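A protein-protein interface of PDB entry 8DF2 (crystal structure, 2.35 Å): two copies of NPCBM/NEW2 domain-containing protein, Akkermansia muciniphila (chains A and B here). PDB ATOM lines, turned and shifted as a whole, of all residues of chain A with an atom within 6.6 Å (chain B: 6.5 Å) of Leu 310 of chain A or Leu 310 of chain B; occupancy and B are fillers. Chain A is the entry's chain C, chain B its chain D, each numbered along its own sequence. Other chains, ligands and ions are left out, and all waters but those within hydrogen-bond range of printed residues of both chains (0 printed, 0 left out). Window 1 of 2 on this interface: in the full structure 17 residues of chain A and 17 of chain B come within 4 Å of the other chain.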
ATOM      1  N   PHE A 307       4.159  17.419 -20.079  1.00  0.00           N
ATOM      2  CA  PHE A 307       2.748  17.302 -19.743  1.00  0.00           C
ATOM      3  C   PHE A 307       1.933  17.117 -21.014  1.00  0.00           C
ATOM      4  O   PHE A 307       2.210  17.753 -22.036  1.00  0.00           O
ATOM      5  CB  PHE A 307       2.253  18.540 -18.996  1.00  0.00           C
ATOM      6  CG  PHE A 307       2.828  18.686 -17.627  1.00  0.00           C
ATOM      7  CD1 PHE A 307       2.195  18.118 -16.538  1.00  0.00           C
ATOM      8  CD2 PHE A 307       4.002  19.392 -17.427  1.00  0.00           C
ATOM      9  CE1 PHE A 307       2.719  18.247 -15.269  1.00  0.00           C
ATOM     10  CE2 PHE A 307       4.535  19.524 -16.168  1.00  0.00           C
ATOM     11  CZ  PHE A 307       3.894  18.952 -15.081  1.00  0.00           C
ATOM     12  N   GLU A 308       0.956  16.207 -20.963  1.00  0.00           N
ATOM     13  CA  GLU A 308      -0.039  16.125 -22.030  1.00  0.00           C
ATOM     14  C   GLU A 308      -1.162  17.130 -21.817  1.00  0.00           C
ATOM     15  O   GLU A 308      -1.801  17.553 -22.784  1.00  0.00           O
ATOM     16  CB  GLU A 308      -0.614  14.710 -22.119  1.00  0.00           C
ATOM     17  CG  GLU A 308       0.368  13.661 -22.645  1.00  0.00           C
ATOM     18  CD  GLU A 308      -0.203  12.245 -22.638  1.00  0.00           C
ATOM     19  OE1 GLU A 308      -1.435  12.089 -22.478  1.00  0.00           O
ATOM     20  OE2 GLU A 308       0.583  11.286 -22.805  1.00  0.00           O
ATOM     21  N   ARG A 309      -1.424  17.495 -20.561  1.00  0.00           N
ATOM     22  CA  ARG A 309      -2.442  18.465 -20.189  1.00  0.00           C
ATOM     23  C   ARG A 309      -1.997  19.119 -18.890  1.00  0.00           C
ATOM     24  O   ARG A 309      -1.490  18.444 -17.994  1.00  0.00           O
ATOM     25  CB  ARG A 309      -3.823  17.804 -20.020  1.00  0.00           C
ATOM     26  CG  ARG A 309      -4.964  18.784 -19.694  1.00  0.00           C
ATOM     27  CD  ARG A 309      -6.333  18.098 -19.576  1.00  0.00           C
ATOM     28  NE  ARG A 309      -6.221  16.790 -18.945  1.00  0.00           N
ATOM     29  CZ  ARG A 309      -6.357  16.562 -17.644  1.00  0.00           C
ATOM     30  NH1 ARG A 309      -6.629  17.540 -16.792  1.00  0.00           N
ATOM     31  NH2 ARG A 309      -6.193  15.322 -17.183  1.00  0.00           N
ATOM     32  N   LEU A 310      -2.178  20.431 -18.797  1.00  0.00           N
ATOM     33  CA  LEU A 310      -1.784  21.170 -17.601  1.00  0.00           C
ATOM     34  C   LEU A 310      -2.724  22.351 -17.424  1.00  0.00           C
ATOM     35  O   LEU A 310      -2.864  23.173 -18.335  1.00  0.00           O
ATOM     36  CB  LEU A 310      -0.339  21.648 -17.700  1.00  0.00           C
ATOM     37  CG  LEU A 310       0.168  22.406 -16.474  1.00  0.00           C
ATOM     38  CD1 LEU A 310       0.209  21.514 -15.241  1.00  0.00           C
ATOM     39  CD2 LEU A 310       1.533  22.985 -16.774  1.00  0.00           C
ATOM     40  N   GLU A 311      -3.356  22.438 -16.255  1.00  0.00           N
ATOM     41  CA  GLU A 311      -4.347  23.467 -15.976  1.00  0.00           C
ATOM     42  C   GLU A 311      -4.088  24.061 -14.602  1.00  0.00           C
ATOM     43  O   GLU A 311      -3.985  23.324 -13.618  1.00  0.00           O
ATOM     44  CB  GLU A 311      -5.771  22.896 -16.042  1.00  0.00           C
ATOM     45  CG  GLU A 311      -6.191  22.392 -17.414  1.00  0.00           C
ATOM     46  CD  GLU A 311      -7.388  21.459 -17.347  1.00  0.00           C
ATOM     47  OE1 GLU A 311      -7.198  20.257 -17.073  1.00  0.00           O
ATOM     48  OE2 GLU A 311      -8.526  21.936 -17.554  1.00  0.00           O
ATOM     49  N   ALA A 312      -3.967  25.386 -14.541  1.00  0.00           N
ATOM     50  CA  ALA A 312      -3.842  26.113 -13.280  1.00  0.00           C
ATOM     51  C   ALA A 312      -5.053  27.037 -13.172  1.00  0.00           C
ATOM     52  O   ALA A 312      -5.099  28.087 -13.817  1.00  0.00           O
ATOM     53  CB  ALA A 312      -2.530  26.888 -13.217  1.00  0.00           C
ATOM     54  N   ILE A 313      -6.032  26.650 -12.368  1.00  0.00           N
ATOM     55  CA  ILE A 313      -7.309  27.352 -12.261  1.00  0.00           C
ATOM     56  C   ILE A 313      -7.332  28.098 -10.933  1.00  0.00           C
ATOM     57  O   ILE A 313      -7.104  27.481  -9.887  1.00  0.00           O
ATOM     58  CB  ILE A 313      -8.506  26.388 -12.363  1.00  0.00           C
ATOM     59  CG1 ILE A 313      -8.206  25.249 -13.349  1.00  0.00           C
ATOM     60  CG2 ILE A 313      -9.772  27.143 -12.772  1.00  0.00           C
ATOM     61  CD1 ILE A 313      -8.234  25.661 -14.804  1.00  0.00           C
ATOM     62  N   PRO A 314      -7.610  29.402 -10.923  1.00  0.00           N
ATOM     63  CA  PRO A 314      -7.619  30.143  -9.653  1.00  0.00           C
ATOM     64  C   PRO A 314      -8.825  29.789  -8.796  1.00  0.00           C
ATOM     65  O   PRO A 314      -9.914  29.517  -9.301  1.00  0.00           O
ATOM     66  CB  PRO A 314      -7.665  31.616 -10.092  1.00  0.00           C
ATOM     67  CG  PRO A 314      -8.328  31.584 -11.419  1.00  0.00           C
ATOM     68  CD  PRO A 314      -7.904  30.274 -12.075  1.00  0.00           C
ATOM     69  N   LEU A 321      -4.722  22.819  -9.418  1.00  0.00           N
ATOM     70  CA  LEU A 321      -3.759  22.337 -10.399  1.00  0.00           C
ATOM     71  C   LEU A 321      -4.152  20.917 -10.781  1.00  0.00           C
ATOM     72  O   LEU A 321      -4.128  20.013  -9.940  1.00  0.00           O
ATOM     73  CB  LEU A 321      -2.342  22.392  -9.837  1.00  0.00           C
ATOM     74  CG  LEU A 321      -1.217  21.985 -10.783  1.00  0.00           C
ATOM     75  CD1 LEU A 321      -1.002  23.081 -11.797  1.00  0.00           C
ATOM     76  CD2 LEU A 321       0.058  21.733 -10.006  1.00  0.00           C
ATOM     77  N   LYS A 322      -4.538  20.727 -12.038  1.00  0.00           N
ATOM     78  CA  LYS A 322      -4.885  19.407 -12.533  1.00  0.00           C
ATOM     79  C   LYS A 322      -4.247  19.236 -13.900  1.00  0.00           C
ATOM     80  O   LYS A 322      -3.891  20.211 -14.566  1.00  0.00           O
ATOM     81  CB  LYS A 322      -6.412  19.202 -12.592  1.00  0.00           C
ATOM     82  CG  LYS A 322      -7.171  20.346 -13.247  1.00  0.00           C
ATOM     83  CD  LYS A 322      -8.674  20.076 -13.316  1.00  0.00           C
ATOM     84  CE  LYS A 322      -9.074  19.532 -14.685  1.00  0.00           C
ATOM     85  NZ  LYS A 322     -10.287  20.208 -15.240  1.00  0.00           N
ATOM     86  N   GLY A 323      -4.070  17.985 -14.304  1.00  0.00           N
ATOM     87  CA  GLY A 323      -3.501  17.735 -15.612  1.00  0.00           C
ATOM     88  C   GLY A 323      -3.107  16.284 -15.774  1.00  0.00           C
ATOM     89  O   GLY A 323      -3.578  15.410 -15.043  1.00  0.00           O
ATOM     90  N   ARG A 324      -2.260  16.048 -16.771  1.00  0.00           N
ATOM     91  CA  ARG A 324      -1.800  14.708 -17.116  1.00  0.00           C
ATOM     92  C   ARG A 324      -0.311  14.776 -17.428  1.00  0.00           C
ATOM     93  O   ARG A 324       0.095  15.373 -18.431  1.00  0.00           O
ATOM     94  CB  ARG A 324      -2.591  14.146 -18.298  1.00  0.00           C
ATOM     95  CG  ARG A 324      -2.343  12.670 -18.608  1.00  0.00           C
ATOM     96  CD  ARG A 324      -3.203  12.225 -19.791  1.00  0.00           C
ATOM     97  NE  ARG A 324      -2.852  10.896 -20.281  1.00  0.00           N
ATOM     98  CZ  ARG A 324      -3.634  10.151 -21.055  1.00  0.00           C
ATOM     99  N   PHE A 361      -3.441  13.791 -12.458  1.00  0.00           N
ATOM    100  CA  PHE A 361      -3.338  14.301 -11.101  1.00  0.00           C
ATOM    101  C   PHE A 361      -4.339  15.437 -10.947  1.00  0.00           C
ATOM    102  O   PHE A 361      -4.736  16.083 -11.921  1.00  0.00           O
ATOM    103  CB  PHE A 361      -1.912  14.782 -10.785  1.00  0.00           C
ATOM    104  CG  PHE A 361      -1.457  15.910 -11.668  1.00  0.00           C
ATOM    105  CD1 PHE A 361      -0.838  15.650 -12.881  1.00  0.00           C
ATOM    106  CD2 PHE A 361      -1.682  17.230 -11.301  1.00  0.00           C
ATOM    107  CE1 PHE A 361      -0.439  16.685 -13.707  1.00  0.00           C
ATOM    108  CE2 PHE A 361      -1.288  18.273 -12.120  1.00  0.00           C
ATOM    109  CZ  PHE A 361      -0.664  18.003 -13.324  1.00  0.00           C
ATOM    110  N   MET A 377       5.187  29.144  -8.270  1.00  0.00           N
ATOM    111  CA  MET A 377       4.694  27.776  -8.141  1.00  0.00           C
ATOM    112  C   MET A 377       5.686  26.812  -8.769  1.00  0.00           C
ATOM    113  O   MET A 377       5.964  26.898  -9.969  1.00  0.00           O
ATOM    114  CB  MET A 377       3.317  27.586  -8.785  1.00  0.00           C
ATOM    115  CG  MET A 377       2.756  26.164  -8.578  1.00  0.00           C
ATOM    116  SD  MET A 377       0.996  25.965  -8.929  1.00  0.00           S
ATOM    117  CE  MET A 377       1.031  26.029 -10.709  1.00  0.00           C
ATOM    118  N   VAL A 379       6.302  22.783  -9.598  1.00  0.00           N
ATOM    119  CA  VAL A 379       5.603  21.515  -9.793  1.00  0.00           C
ATOM    120  C   VAL A 379       6.653  20.445 -10.064  1.00  0.00           C
ATOM    121  O   VAL A 379       7.405  20.541 -11.044  1.00  0.00           O
ATOM    122  CB  VAL A 379       4.585  21.583 -10.938  1.00  0.00           C
ATOM    123  CG1 VAL A 379       3.865  20.254 -11.056  1.00  0.00           C
ATOM    124  CG2 VAL A 379       3.598  22.720 -10.707  1.00  0.00           C
ATOM    125  N   ILE A 391       8.981  21.952 -13.158  1.00  0.00           N
ATOM    126  CA  ILE A 391       8.755  23.183 -13.901  1.00  0.00           C
ATOM    127  C   ILE A 391       8.406  24.270 -12.892  1.00  0.00           C
ATOM    128  O   ILE A 391       8.034  23.997 -11.748  1.00  0.00           O
ATOM    129  CB  ILE A 391       7.648  23.049 -14.971  1.00  0.00           C
ATOM    130  CG1 ILE A 391       6.310  22.703 -14.321  1.00  0.00           C
ATOM    131  CG2 ILE A 391       8.024  21.997 -16.011  1.00  0.00           C
ATOM    132  CD1 ILE A 391       5.101  22.983 -15.209  1.00  0.00           C
ATOM    133  N   LEU A 393       6.201  28.006 -12.600  1.00  0.00           N
ATOM    134  CA  LEU A 393       5.195  28.861 -13.205  1.00  0.00           C
ATOM    135  C   LEU A 393       5.034  30.148 -12.408  1.00  0.00           C
ATOM    136  O   LEU A 393       5.022  30.115 -11.172  1.00  0.00           O
ATOM    137  CB  LEU A 393       3.844  28.147 -13.287  1.00  0.00           C
ATOM    138  CG  LEU A 393       3.713  27.170 -14.454  1.00  0.00           C
ATOM    139  CD1 LEU A 393       2.266  26.758 -14.615  1.00  0.00           C
ATOM    140  CD2 LEU A 393       4.262  27.773 -15.743  1.00  0.00           C
ATOM    141  N   PRO A 394       4.952  31.294 -13.078  1.00  0.00           N
ATOM    142  CA  PRO A 394       4.664  32.541 -12.365  1.00  0.00           C
ATOM    143  C   PRO A 394       3.167  32.783 -12.244  1.00  0.00           C
ATOM    144  O   PRO A 394       2.448  32.853 -13.251  1.00  0.00           O
ATOM    145  CB  PRO A 394       5.354  33.600 -13.232  1.00  0.00           C
ATOM    146  CG  PRO A 394       5.390  32.996 -14.629  1.00  0.00           C
ATOM    147  CD  PRO A 394       5.128  31.515 -14.524  1.00  0.00           C
ATOM    148  N   PHE B 307       0.590  34.709 -14.435  1.00  0.00           N
ATOM    149  CA  PHE B 307      -0.721  34.277 -14.891  1.00  0.00           C
ATOM    150  C   PHE B 307      -1.647  34.076 -13.699  1.00  0.00           C
ATOM    151  O   PHE B 307      -1.248  33.509 -12.675  1.00  0.00           O
ATOM    152  CB  PHE B 307      -0.627  32.970 -15.695  1.00  0.00           C
ATOM    153  CG  PHE B 307       0.089  33.112 -17.014  1.00  0.00           C
ATOM    154  CD1 PHE B 307       1.470  33.062 -17.075  1.00  0.00           C
ATOM    155  CD2 PHE B 307      -0.622  33.278 -18.196  1.00  0.00           C
ATOM    156  CE1 PHE B 307       2.135  33.192 -18.286  1.00  0.00           C
ATOM    157  CE2 PHE B 307       0.041  33.406 -19.412  1.00  0.00           C
ATOM    158  CZ  PHE B 307       1.420  33.365 -19.453  1.00  0.00           C
ATOM    159  N   GLU B 308      -2.884  34.555 -13.835  1.00  0.00           N
ATOM    160  CA  GLU B 308      -3.922  34.191 -12.878  1.00  0.00           C
ATOM    161  C   GLU B 308      -4.542  32.843 -13.222  1.00  0.00           C
ATOM    162  O   GLU B 308      -4.989  32.122 -12.326  1.00  0.00           O
ATOM    163  CB  GLU B 308      -5.011  35.264 -12.834  1.00  0.00           C
ATOM    164  CG  GLU B 308      -4.507  36.680 -13.005  1.00  0.00           C
ATOM    165  CD  GLU B 308      -5.558  37.738 -12.676  1.00  0.00           C
ATOM    166  OE1 GLU B 308      -6.771  37.440 -12.749  1.00  0.00           O
ATOM    167  OE2 GLU B 308      -5.164  38.880 -12.349  1.00  0.00           O
ATOM    168  N   ARG B 309      -4.551  32.480 -14.504  1.00  0.00           N
ATOM    169  CA  ARG B 309      -5.092  31.207 -14.957  1.00  0.00           C
ATOM    170  C   ARG B 309      -4.335  30.796 -16.211  1.00  0.00           C
ATOM    171  O   ARG B 309      -4.067  31.637 -17.072  1.00  0.00           O
ATOM    172  CB  ARG B 309      -6.599  31.309 -15.242  1.00  0.00           C
ATOM    173  CG  ARG B 309      -7.266  29.985 -15.622  1.00  0.00           C
ATOM    174  CD  ARG B 309      -8.788  30.144 -15.749  1.00  0.00           C
ATOM    175  NE  ARG B 309      -9.140  31.408 -16.385  1.00  0.00           N
ATOM    176  CZ  ARG B 309      -9.252  31.590 -17.695  1.00  0.00           C
ATOM    177  NH1 ARG B 309      -9.067  30.599 -18.552  1.00  0.00           N
ATOM    178  NH2 ARG B 309      -9.548  32.801 -18.159  1.00  0.00           N
ATOM    179  N   LEU B 310      -3.998  29.508 -16.312  1.00  0.00           N
ATOM    180  CA  LEU B 310      -3.266  28.999 -17.470  1.00  0.00           C
ATOM    181  C   LEU B 310      -3.694  27.565 -17.747  1.00  0.00           C
ATOM    182  O   LEU B 310      -3.625  26.711 -16.858  1.00  0.00           O
ATOM    183  CB  LEU B 310      -1.753  29.075 -17.239  1.00  0.00           C
ATOM    184  CG  LEU B 310      -0.850  28.688 -18.414  1.00  0.00           C
ATOM    185  CD1 LEU B 310      -1.051  29.618 -19.596  1.00  0.00           C
ATOM    186  CD2 LEU B 310       0.626  28.655 -18.005  1.00  0.00           C
ATOM    187  N   GLU B 311      -4.152  27.303 -18.971  1.00  0.00           N
ATOM    188  CA  GLU B 311      -4.656  25.987 -19.341  1.00  0.00           C
ATOM    189  C   GLU B 311      -4.118  25.586 -20.702  1.00  0.00           C
ATOM    190  O   GLU B 311      -4.312  26.304 -21.687  1.00  0.00           O
ATOM    191  CB  GLU B 311      -6.186  25.970 -19.358  1.00  0.00           C
ATOM    192  CG  GLU B 311      -6.811  26.692 -18.170  1.00  0.00           C
ATOM    193  CD  GLU B 311      -8.306  26.784 -18.266  1.00  0.00           C
ATOM    194  OE1 GLU B 311      -8.938  25.804 -18.721  1.00  0.00           O
ATOM    195  OE2 GLU B 311      -8.850  27.839 -17.889  1.00  0.00           O
ATOM    196  N   ALA B 312      -3.484  24.420 -20.757  1.00  0.00           N
ATOM    197  CA  ALA B 312      -2.978  23.830 -21.995  1.00  0.00           C
ATOM    198  C   ALA B 312      -3.756  22.534 -22.200  1.00  0.00           C
ATOM    199  O   ALA B 312      -3.478  21.537 -21.530  1.00  0.00           O
ATOM    200  CB  ALA B 312      -1.475  23.580 -21.913  1.00  0.00           C
ATOM    201  N   ILE B 313      -4.725  22.551 -23.111  1.00  0.00           N
ATOM    202  CA  ILE B 313      -5.661  21.442 -23.291  1.00  0.00           C
ATOM    203  C   ILE B 313      -5.280  20.691 -24.561  1.00  0.00           C
ATOM    204  O   ILE B 313      -5.242  21.304 -25.636  1.00  0.00           O
ATOM    205  CB  ILE B 313      -7.116  21.926 -23.372  1.00  0.00           C
ATOM    206  CG1 ILE B 313      -7.385  23.004 -22.320  1.00  0.00           C
ATOM    207  CG2 ILE B 313      -8.075  20.741 -23.213  1.00  0.00           C
ATOM    208  CD1 ILE B 313      -7.299  22.500 -20.906  1.00  0.00           C
ATOM    209  N   PRO B 314      -5.037  19.388 -24.496  1.00  0.00           N
ATOM    210  CA  PRO B 314      -4.651  18.671 -25.713  1.00  0.00           C
ATOM    211  C   PRO B 314      -5.842  18.501 -26.633  1.00  0.00           C
ATOM    212  O   PRO B 314      -6.971  18.274 -26.189  1.00  0.00           O
ATOM    213  CB  PRO B 314      -4.145  17.322 -25.189  1.00  0.00           C
ATOM    214  CG  PRO B 314      -4.820  17.149 -23.864  1.00  0.00           C
ATOM    215  CD  PRO B 314      -5.040  18.520 -23.303  1.00  0.00           C
ATOM    216  N   LEU B 321      -4.569  26.677 -25.924  1.00  0.00           N
ATOM    217  CA  LEU B 321      -3.943  27.442 -24.852  1.00  0.00           C
ATOM    218  C   LEU B 321      -4.868  28.597 -24.507  1.00  0.00           C
ATOM    219  O   LEU B 321      -5.103  29.476 -25.339  1.00  0.00           O
ATOM    220  CB  LEU B 321      -2.562  27.945 -25.274  1.00  0.00           C
ATOM    221  CG  LEU B 321      -1.753  28.730 -24.241  1.00  0.00           C
ATOM    222  CD1 LEU B 321      -1.253  27.815 -23.134  1.00  0.00           C
ATOM    223  CD2 LEU B 321      -0.589  29.435 -24.915  1.00  0.00           C
ATOM    224  N   LYS B 322      -5.419  28.577 -23.299  1.00  0.00           N
ATOM    225  CA  LYS B 322      -6.282  29.654 -22.840  1.00  0.00           C
ATOM    226  C   LYS B 322      -5.921  29.982 -21.401  1.00  0.00           C
ATOM    227  O   LYS B 322      -5.307  29.175 -20.695  1.00  0.00           O
ATOM    228  CB  LYS B 322      -7.773  29.285 -22.979  1.00  0.00           C
ATOM    229  CG  LYS B 322      -8.228  28.127 -22.100  1.00  0.00           C
ATOM    230  CD  LYS B 322      -9.720  27.803 -22.270  1.00  0.00           C
ATOM    231  CE  LYS B 322     -10.369  27.511 -20.906  1.00  0.00           C
ATOM    232  NZ  LYS B 322     -11.228  26.284 -20.872  1.00  0.00           N
ATOM    233  N   GLY B 323      -6.274  31.192 -20.982  1.00  0.00           N
ATOM    234  CA  GLY B 323      -6.011  31.590 -19.612  1.00  0.00           C
ATOM    235  C   GLY B 323      -6.184  33.084 -19.420  1.00  0.00           C
ATOM    236  O   GLY B 323      -6.809  33.770 -20.234  1.00  0.00           O
ATOM    237  N   ARG B 324      -5.618  33.574 -18.321  1.00  0.00           N
ATOM    238  CA  ARG B 324      -5.735  34.979 -17.949  1.00  0.00           C
ATOM    239  C   ARG B 324      -4.367  35.463 -17.497  1.00  0.00           C
ATOM    240  O   ARG B 324      -3.849  34.996 -16.476  1.00  0.00           O
ATOM    241  CB  ARG B 324      -6.771  35.187 -16.846  1.00  0.00           C
ATOM    242  CG  ARG B 324      -7.092  36.644 -16.576  1.00  0.00           C
ATOM    243  CD  ARG B 324      -8.261  36.772 -15.603  1.00  0.00           C
ATOM    244  NE  ARG B 324      -8.541  38.165 -15.280  1.00  0.00           N
ATOM    245  CZ  ARG B 324      -9.651  38.598 -14.696  1.00  0.00           C
ATOM    246  NH1 ARG B 324     -10.624  37.766 -14.353  1.00  0.00           N
ATOM    247  NH2 ARG B 324      -9.791  39.898 -14.454  1.00  0.00           N
ATOM    248  N   PHE B 361      -7.242  35.237 -22.915  1.00  0.00           N
ATOM    249  CA  PHE B 361      -6.842  34.846 -24.258  1.00  0.00           C
ATOM    250  C   PHE B 361      -7.300  33.417 -24.504  1.00  0.00           C
ATOM    251  O   PHE B 361      -7.540  32.646 -23.567  1.00  0.00           O
ATOM    252  CB  PHE B 361      -5.325  34.974 -24.467  1.00  0.00           C
ATOM    253  CG  PHE B 361      -4.509  34.138 -23.523  1.00  0.00           C
ATOM    254  CD1 PHE B 361      -4.210  34.599 -22.247  1.00  0.00           C
ATOM    255  CD2 PHE B 361      -4.051  32.887 -23.906  1.00  0.00           C
ATOM    256  CE1 PHE B 361      -3.472  33.836 -21.376  1.00  0.00           C
ATOM    257  CE2 PHE B 361      -3.298  32.112 -23.033  1.00  0.00           C
ATOM    258  CZ  PHE B 361      -3.008  32.586 -21.769  1.00  0.00           C
ATOM    259  N   MET B 377       6.905  24.427 -25.965  1.00  0.00           N
ATOM    260  CA  MET B 377       5.962  25.522 -26.156  1.00  0.00           C
ATOM    261  C   MET B 377       6.462  26.770 -25.443  1.00  0.00           C
ATOM    262  O   MET B 377       6.636  26.763 -24.220  1.00  0.00           O
ATOM    263  CB  MET B 377       4.563  25.170 -25.661  1.00  0.00           C
ATOM    264  CG  MET B 377       3.539  26.184 -26.118  1.00  0.00           C
ATOM    265  SD  MET B 377       1.815  25.738 -25.894  1.00  0.00           S
ATOM    266  CE  MET B 377       1.652  25.916 -24.128  1.00  0.00           C
ATOM    267  N   VAL B 379       5.493  30.737 -24.602  1.00  0.00           N
ATOM    268  CA  VAL B 379       4.347  31.633 -24.491  1.00  0.00           C
ATOM    269  C   VAL B 379       4.873  33.028 -24.180  1.00  0.00           C
ATOM    270  O   VAL B 379       5.535  33.229 -23.155  1.00  0.00           O
ATOM    271  CB  VAL B 379       3.362  31.159 -23.414  1.00  0.00           C
ATOM    272  CG1 VAL B 379       2.231  32.161 -23.267  1.00  0.00           C
ATOM    273  CG2 VAL B 379       2.833  29.761 -23.762  1.00  0.00           C
ATOM    274  N   ILE B 391       7.215  32.492 -20.778  1.00  0.00           N
ATOM    275  CA  ILE B 391       7.379  31.246 -20.045  1.00  0.00           C
ATOM    276  C   ILE B 391       7.574  30.148 -21.083  1.00  0.00           C
ATOM    277  O   ILE B 391       7.219  30.301 -22.254  1.00  0.00           O
ATOM    278  CB  ILE B 391       6.168  30.919 -19.143  1.00  0.00           C
ATOM    279  CG1 ILE B 391       4.905  30.782 -19.995  1.00  0.00           C
ATOM    280  CG2 ILE B 391       5.977  31.985 -18.074  1.00  0.00           C
ATOM    281  CD1 ILE B 391       3.913  29.746 -19.487  1.00  0.00           C
ATOM    282  N   LEU B 393       7.062  25.852 -21.572  1.00  0.00           N
ATOM    283  CA  LEU B 393       6.444  24.649 -21.054  1.00  0.00           C
ATOM    284  C   LEU B 393       6.875  23.441 -21.875  1.00  0.00           C
ATOM    285  O   LEU B 393       6.939  23.517 -23.108  1.00  0.00           O
ATOM    286  CB  LEU B 393       4.918  24.748 -21.074  1.00  0.00           C
ATOM    287  CG  LEU B 393       4.308  25.673 -20.024  1.00  0.00           C
ATOM    288  CD1 LEU B 393       2.815  25.861 -20.282  1.00  0.00           C
ATOM    289  CD2 LEU B 393       4.562  25.136 -18.625  1.00  0.00           C
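Leu 310 of chain A touches three residues of chain B.
Printed residues of chain B within 4 Å of Ile 313 of chain A: Glu 311 (3.6 Å).
Printed residues of chain B within 4 Å of Pro 394 of chain A: Phe 307 (2.9 Å) and Ile 391 (3.6 Å).
Of the printed residues of chain A, Phe 307 of chain B touches Pro 394.
Printed residues of chain A within 4 Å of Arg 309 of chain B: Ala 312 (3.3 Å) and Pro 314 (3.6 Å).
Leu 310 of chain B touches just these residues of chain A: Leu 310, Glu 311 and Ala 312.
The nearest residue of chain A that does not touch Leu 310 of chain B is Leu 393 of chain A (4.2 Å).
Glu 308 of chain A touches Pro 314 of chain B (O to CG, 3.2 Å).
Arg 309 of chain A touches Ala 312 of chain B.
Pro 314 of chain B touches Arg 309 of chain A.
Leu 310 of chain B touches Leu 310 of chain A.
Glu 311 of chain B touches Leu 310 of chain A.
CA of Glu 311 of chain A touches O of Leu 310 of chain B (3.4 Å).
OE2 of Glu 311 of chain A touches CD1 of Ile 313 of chain B, at 3.6 Å.
Ala 312 of chain A touches Arg 309 of chain B.
Arg 309 of chain B touches Pro 314 of chain A (CB to CD, 3.6 Å).
Ile 391 of chain B touches Pro 394 of chain A.
Glu 308 of chain A touches Pro 314 of chain B, and with the chains exchanged Pro 314 of chain A touches Glu 308 of chain B.
Leu 310 of chain A touches Glu 311 of chain B, and with the chains exchanged Glu 311 of chain A touches Leu 310 of chain B.
Leu 310 of chain A touches Ala 312 of chain B, and with the chains exchanged Ala 312 of chain A touches Leu 310 of chain B.
Leu 393 of chain A touches its own counterpart, Leu 393 of chain B.
Positions printed for both chains: 307, 308, 309, 310, 311, 312, 313, 314, 321, 322, 323, 324, 361, 377, 379, 391 and 393.
The side-chain carboxylate (OE2) of Glu 311 of chain A lies within salt-bridge range of the side-chain amino group (NZ) of Lys 322 of chain A (3.4 Å).
NH1 of Arg 309 of chain A is in salt-bridge range of OE1 of Glu 311 of chain A (2.8 Å).
O of Arg 309 of chain A lies within hydrogen-bond range of N of Arg 324 of chain A (2.8 Å).
The guanidinium group of Arg 309 of chain A is in hydrogen-bond range of the backbone carbonyl oxygen of Gly 323 of chain A (3.4 Å).
OE2 of Glu 311 of chain B is in salt-bridge range of NH1 of Arg 309 of chain B (2.8 Å).
NE of Arg 324 of chain B is in salt-bridge range of OE1 of Glu 308 of chain B, 3.2 Å away.
Of the 18 printed residues of chain A, 9 touch a printed residue of chain B.
Of the 17 printed residues of chain B, 10 touch a printed residue of chain A.
Among the printed residues, no Asp or Glu carboxylate lies within 4 Å of a Lys or Arg side-chain nitrogen of the other chain.
The backbone NH (N) of Ala 312 of chain A sits at hydrogen-bond distance from the backbone carbonyl oxygen (O) of Leu 310 of chain B, 2.7 Å away.
N of Ala 312 of chain B sits at hydrogen-bond distance from O of Leu 310 of chain A, 2.8 Å away.
The backbone carbonyl oxygen (O) of Pro 394 of chain A sits at hydrogen-bond distance from the backbone NH (N) of Phe 307 of chain B (2.9 Å).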
